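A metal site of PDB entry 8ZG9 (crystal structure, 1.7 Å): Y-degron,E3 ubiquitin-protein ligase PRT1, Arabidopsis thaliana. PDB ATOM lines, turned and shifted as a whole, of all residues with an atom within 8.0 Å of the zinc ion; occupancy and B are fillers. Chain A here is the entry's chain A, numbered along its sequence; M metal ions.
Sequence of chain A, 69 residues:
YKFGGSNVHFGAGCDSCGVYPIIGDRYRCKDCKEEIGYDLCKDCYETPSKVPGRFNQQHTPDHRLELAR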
ATOM      1  N   GLY A  13      25.354 -14.370  13.567  1.00  0.00           N
ATOM      2  CA  GLY A  13      25.995 -14.520  14.856  1.00  0.00           C
ATOM      3  C   GLY A  13      24.982 -14.531  15.975  1.00  0.00           C
ATOM      4  O   GLY A  13      23.878 -13.988  15.815  1.00  0.00           O
ATOM      5  N   CYS A  14      25.336 -15.140  17.096  1.00  0.00           N
ATOM      6  CA  CYS A  14      24.441 -15.236  18.253  1.00  0.00           C
ATOM      7  C   CYS A  14      24.519 -13.962  19.081  1.00  0.00           C
ATOM      8  O   CYS A  14      25.597 -13.571  19.535  1.00  0.00           O
ATOM      9  CB  CYS A  14      24.786 -16.454  19.106  1.00  0.00           C
ATOM     10  SG  CYS A  14      23.752 -16.624  20.576  1.00  0.00           S
ATOM     11  N   ASP A  15      23.370 -13.310  19.284  1.00  0.00           N
ATOM     12  CA  ASP A  15      23.343 -12.072  20.048  1.00  0.00           C
ATOM     13  C   ASP A  15      23.606 -12.281  21.536  1.00  0.00           C
ATOM     14  O   ASP A  15      23.918 -11.314  22.241  1.00  0.00           O
ATOM     15  CB  ASP A  15      21.984 -11.394  19.874  1.00  0.00           C
ATOM     16  CG  ASP A  15      21.872 -10.617  18.567  1.00  0.00           C
ATOM     17  OD1 ASP A  15      22.380  -9.478  18.480  1.00  0.00           O
ATOM     18  OD2 ASP A  15      21.295 -11.166  17.603  1.00  0.00           O
ATOM     19  N   SER A  16      23.552 -13.532  22.017  1.00  0.00           N
ATOM     20  CA  SER A  16      23.793 -13.808  23.430  1.00  0.00           C
ATOM     21  C   SER A  16      25.259 -14.141  23.696  1.00  0.00           C
ATOM     22  O   SER A  16      25.941 -13.404  24.417  1.00  0.00           O
ATOM     23  CB  SER A  16      22.918 -14.987  23.879  1.00  0.00           C
ATOM     24  OG  SER A  16      23.252 -15.402  25.188  1.00  0.00           O
ATOM     25  N   CYS A  17      25.760 -15.206  23.071  1.00  0.00           N
ATOM     26  CA  CYS A  17      27.122 -15.673  23.325  1.00  0.00           C
ATOM     27  C   CYS A  17      28.115 -15.124  22.317  1.00  0.00           C
ATOM     28  O   CYS A  17      29.326 -15.164  22.573  1.00  0.00           O
ATOM     29  CB  CYS A  17      27.125 -17.201  23.322  1.00  0.00           C
ATOM     30  SG  CYS A  17      27.017 -17.972  21.710  1.00  0.00           S
ATOM     31  N   GLY A  18      27.641 -14.587  21.187  1.00  0.00           N
ATOM     32  CA  GLY A  18      28.469 -13.930  20.201  1.00  0.00           C
ATOM     33  C   GLY A  18      29.070 -14.844  19.159  1.00  0.00           C
ATOM     34  O   GLY A  18      29.776 -14.352  18.269  1.00  0.00           O
ATOM     35  N   VAL A  19      28.810 -16.150  19.230  1.00  0.00           N
ATOM     36  CA  VAL A  19      29.415 -17.064  18.277  1.00  0.00           C
ATOM     37  C   VAL A  19      29.015 -16.694  16.853  1.00  0.00           C
ATOM     38  O   VAL A  19      27.866 -16.324  16.591  1.00  0.00           O
ATOM     39  CB  VAL A  19      29.036 -18.526  18.580  1.00  0.00           C
ATOM     40  CG1 VAL A  19      27.559 -18.758  18.316  1.00  0.00           C
ATOM     41  CG2 VAL A  19      29.883 -19.467  17.742  1.00  0.00           C
ATOM     42  N   TYR A  20      29.978 -16.763  15.954  1.00  0.00           N
ATOM     43  CA  TYR A  20      29.787 -16.432  14.551  1.00  0.00           C
ATOM     44  C   TYR A  20      30.805 -17.163  13.690  1.00  0.00           C
ATOM     45  O   TYR A  20      32.019 -17.076  13.935  1.00  0.00           O
ATOM     46  CB  TYR A  20      29.858 -14.921  14.352  1.00  0.00           C
ATOM     47  CG  TYR A  20      29.763 -14.452  12.925  1.00  0.00           C
ATOM     48  CD1 TYR A  20      30.735 -14.794  11.985  1.00  0.00           C
ATOM     49  CD2 TYR A  20      28.687 -13.696  12.514  1.00  0.00           C
ATOM     50  CE1 TYR A  20      30.637 -14.341  10.676  1.00  0.00           C
ATOM     51  CE2 TYR A  20      28.578 -13.262  11.208  1.00  0.00           C
ATOM     52  CZ  TYR A  20      29.560 -13.578  10.310  1.00  0.00           C
ATOM     53  OH  TYR A  20      29.455 -13.136   9.007  1.00  0.00           O
ATOM     54  N   ILE A  22      26.912 -19.024  13.428  1.00  0.00           N
ATOM     55  CA  ILE A  22      26.213 -20.009  14.251  1.00  0.00           C
ATOM     56  C   ILE A  22      26.365 -21.383  13.598  1.00  0.00           C
ATOM     57  O   ILE A  22      26.070 -21.562  12.409  1.00  0.00           O
ATOM     58  CB  ILE A  22      24.737 -19.629  14.420  1.00  0.00           C
ATOM     59  CG1 ILE A  22      24.610 -18.344  15.235  1.00  0.00           C
ATOM     60  CG2 ILE A  22      23.967 -20.773  15.065  1.00  0.00           C
ATOM     61  CD1 ILE A  22      23.210 -17.757  15.272  1.00  0.00           C
ATOM     62  N   ASP A  25      21.716 -25.521  15.119  1.00  0.00           N
ATOM     63  CA  ASP A  25      20.428 -24.863  14.952  1.00  0.00           C
ATOM     64  C   ASP A  25      20.513 -23.381  15.274  1.00  0.00           C
ATOM     65  O   ASP A  25      21.200 -22.950  16.214  1.00  0.00           O
ATOM     66  CB  ASP A  25      19.354 -25.515  15.829  1.00  0.00           C
ATOM     67  CG  ASP A  25      18.958 -26.888  15.341  1.00  0.00           C
ATOM     68  OD1 ASP A  25      19.210 -27.205  14.151  1.00  0.00           O
ATOM     69  OD2 ASP A  25      18.364 -27.664  16.124  1.00  0.00           O
ATOM     70  N   ASP A  39      19.275 -13.046  16.576  1.00  0.00           N
ATOM     71  CA  ASP A  39      19.398 -14.494  16.462  1.00  0.00           C
ATOM     72  C   ASP A  39      20.033 -15.073  17.713  1.00  0.00           C
ATOM     73  O   ASP A  39      20.804 -14.409  18.407  1.00  0.00           O
ATOM     74  CB  ASP A  39      20.251 -14.922  15.256  1.00  0.00           C
ATOM     75  CG  ASP A  39      19.774 -14.324  13.957  1.00  0.00           C
ATOM     76  OD1 ASP A  39      20.168 -13.180  13.665  1.00  0.00           O
ATOM     77  OD2 ASP A  39      19.024 -15.011  13.236  1.00  0.00           O
ATOM     78  N   LEU A  40      19.709 -16.327  17.974  1.00  0.00           N
ATOM     79  CA  LEU A  40      20.324 -17.084  19.043  1.00  0.00           C
ATOM     80  C   LEU A  40      20.765 -18.440  18.510  1.00  0.00           C
ATOM     81  O   LEU A  40      20.105 -19.034  17.645  1.00  0.00           O
ATOM     82  CB  LEU A  40      19.361 -17.302  20.206  1.00  0.00           C
ATOM     83  CG  LEU A  40      18.835 -16.060  20.937  1.00  0.00           C
ATOM     84  CD1 LEU A  40      17.716 -16.436  21.927  1.00  0.00           C
ATOM     85  CD2 LEU A  40      19.959 -15.339  21.631  1.00  0.00           C
ATOM     86  N   CYS A  41      21.858 -18.944  19.059  1.00  0.00           N
ATOM     87  CA  CYS A  41      22.231 -20.333  18.834  1.00  0.00           C
ATOM     88  C   CYS A  41      21.347 -21.211  19.703  1.00  0.00           C
ATOM     89  O   CYS A  41      20.663 -20.714  20.608  1.00  0.00           O
ATOM     90  CB  CYS A  41      23.708 -20.543  19.158  1.00  0.00           C
ATOM     91  SG  CYS A  41      24.153 -20.449  20.898  1.00  0.00           S
ATOM     92  N   LYS A  42      21.386 -22.522  19.463  1.00  0.00           N
ATOM     93  CA  LYS A  42      20.481 -23.392  20.203  1.00  0.00           C
ATOM     94  C   LYS A  42      20.752 -23.335  21.705  1.00  0.00           C
ATOM     95  O   LYS A  42      19.803 -23.321  22.514  1.00  0.00           O
ATOM     96  CB  LYS A  42      20.590 -24.819  19.689  1.00  0.00           C
ATOM     97  CG  LYS A  42      19.598 -25.756  20.335  1.00  0.00           C
ATOM     98  CD  LYS A  42      19.667 -27.092  19.673  1.00  0.00           C
ATOM     99  CE  LYS A  42      18.444 -27.898  19.994  1.00  0.00           C
ATOM    100  NZ  LYS A  42      18.546 -29.260  19.398  1.00  0.00           N
ATOM    101  N   ASP A  43      22.024 -23.348  22.103  1.00  0.00           N
ATOM    102  CA  ASP A  43      22.356 -23.367  23.520  1.00  0.00           C
ATOM    103  C   ASP A  43      21.802 -22.149  24.257  1.00  0.00           C
ATOM    104  O   ASP A  43      21.207 -22.275  25.332  1.00  0.00           O
ATOM    105  CB  ASP A  43      23.867 -23.452  23.703  1.00  0.00           C
ATOM    106  CG  ASP A  43      24.411 -24.817  23.303  1.00  0.00           C
ATOM    107  OD1 ASP A  43      23.617 -25.778  23.192  1.00  0.00           O
ATOM    108  OD2 ASP A  43      25.651 -24.943  23.115  1.00  0.00           O
ATOM    109  N   CYS A  44      21.969 -20.955  23.672  1.00  0.00           N
ATOM    110  CA  CYS A  44      21.452 -19.732  24.283  1.00  0.00           C
ATOM    111  C   CYS A  44      19.938 -19.686  24.214  1.00  0.00           C
ATOM    112  O   CYS A  44      19.291 -19.109  25.104  1.00  0.00           O
ATOM    113  CB  CYS A  44      22.085 -18.531  23.575  1.00  0.00           C
ATOM    114  SG  CYS A  44      23.884 -18.365  23.871  1.00  0.00           S
ATOM    115  N   TYR A  45      19.342 -20.339  23.213  1.00  0.00           N
ATOM    116  CA  TYR A  45      17.891 -20.421  23.107  1.00  0.00           C
ATOM    117  C   TYR A  45      17.296 -21.274  24.209  1.00  0.00           C
ATOM    118  O   TYR A  45      16.208 -20.984  24.723  1.00  0.00           O
ATOM    119  CB  TYR A  45      17.518 -21.039  21.768  1.00  0.00           C
ATOM    120  CG  TYR A  45      16.061 -21.354  21.522  1.00  0.00           C
ATOM    121  CD1 TYR A  45      15.150 -20.361  21.212  1.00  0.00           C
ATOM    122  CD2 TYR A  45      15.606 -22.676  21.581  1.00  0.00           C
ATOM    123  CE1 TYR A  45      13.823 -20.661  20.960  1.00  0.00           C
ATOM    124  CE2 TYR A  45      14.271 -22.986  21.335  1.00  0.00           C
ATOM    125  CZ  TYR A  45      13.396 -21.973  21.022  1.00  0.00           C
ATOM    126  OH  TYR A  45      12.086 -22.289  20.764  1.00  0.00           O
ATOM    127  N   THR A  47      18.458 -21.662  27.185  1.00  0.00           N
ATOM    128  CA  THR A  47      18.653 -20.987  28.476  1.00  0.00           C
ATOM    129  C   THR A  47      18.304 -19.512  28.362  1.00  0.00           C
ATOM    130  O   THR A  47      19.183 -18.693  28.089  1.00  0.00           O
ATOM    131  CB  THR A  47      20.083 -21.162  28.985  1.00  0.00           C
ATOM    132  OG1 THR A  47      21.059 -20.701  28.022  1.00  0.00           O
ATOM    133  CG2 THR A  47      20.342 -22.662  29.311  1.00  0.00           C
ATOM    134  N   ARG A  54      23.213  -7.362  20.555  1.00  0.00           N
ATOM    135  CA  ARG A  54      24.543  -6.782  20.455  1.00  0.00           C
ATOM    136  C   ARG A  54      24.624  -5.578  19.524  1.00  0.00           C
ATOM    137  O   ARG A  54      25.691  -4.956  19.458  1.00  0.00           O
ATOM    138  CB  ARG A  54      25.528  -7.864  19.987  1.00  0.00           C
ATOM    139  CG  ARG A  54      25.849  -8.905  21.045  1.00  0.00           C
ATOM    140  CD  ARG A  54      26.711 -10.083  20.574  1.00  0.00           C
ATOM    141  NE  ARG A  54      26.923 -10.982  21.718  1.00  0.00           N
ATOM    142  CZ  ARG A  54      28.014 -10.985  22.468  1.00  0.00           C
ATOM    143  NH1 ARG A  54      28.125 -11.822  23.488  1.00  0.00           N
ATOM    144  NH2 ARG A  54      29.024 -10.172  22.186  1.00  0.00           N
HETATM  145 ZN    ZN M   1      24.755 -18.384  21.699  1.00  0.00          ZN
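Four residues have an atom within 4 Å of the zinc ion: Cys 14, Cys 17, Cys 41 and Cys 44. The nearest printed residue that does not touch the zinc ion is Val 19 (4.4 Å).
The zinc ion is bound by SG of Cys 41, at 2.3 Å. SG of Cys 17 binds the zinc ion, at 2.3 Å. The side-chain sulfur (SG) of Cys 14 is bound to the zinc ion (2.3 Å). The side-chain sulfur (SG) of Cys 44 is bound to the zinc ion, at 2.3 Å.
SG of Cys 14 lies close to N of Ser 16. N of Cys 14 is in hydrogen-bond range of O of Val 19 (2.8 Å). The side-chain sulfur (SG) of Cys 41 lies close to the backbone NH (N) of Asp 43, 3.8 Å away. SG of Cys 44 lies close to OG of Ser 16, at 3.3 Å. The backbone NH (N) of Val 19 sits close to the side-chain sulfur (SG) of Cys 17 (3.6 Å).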
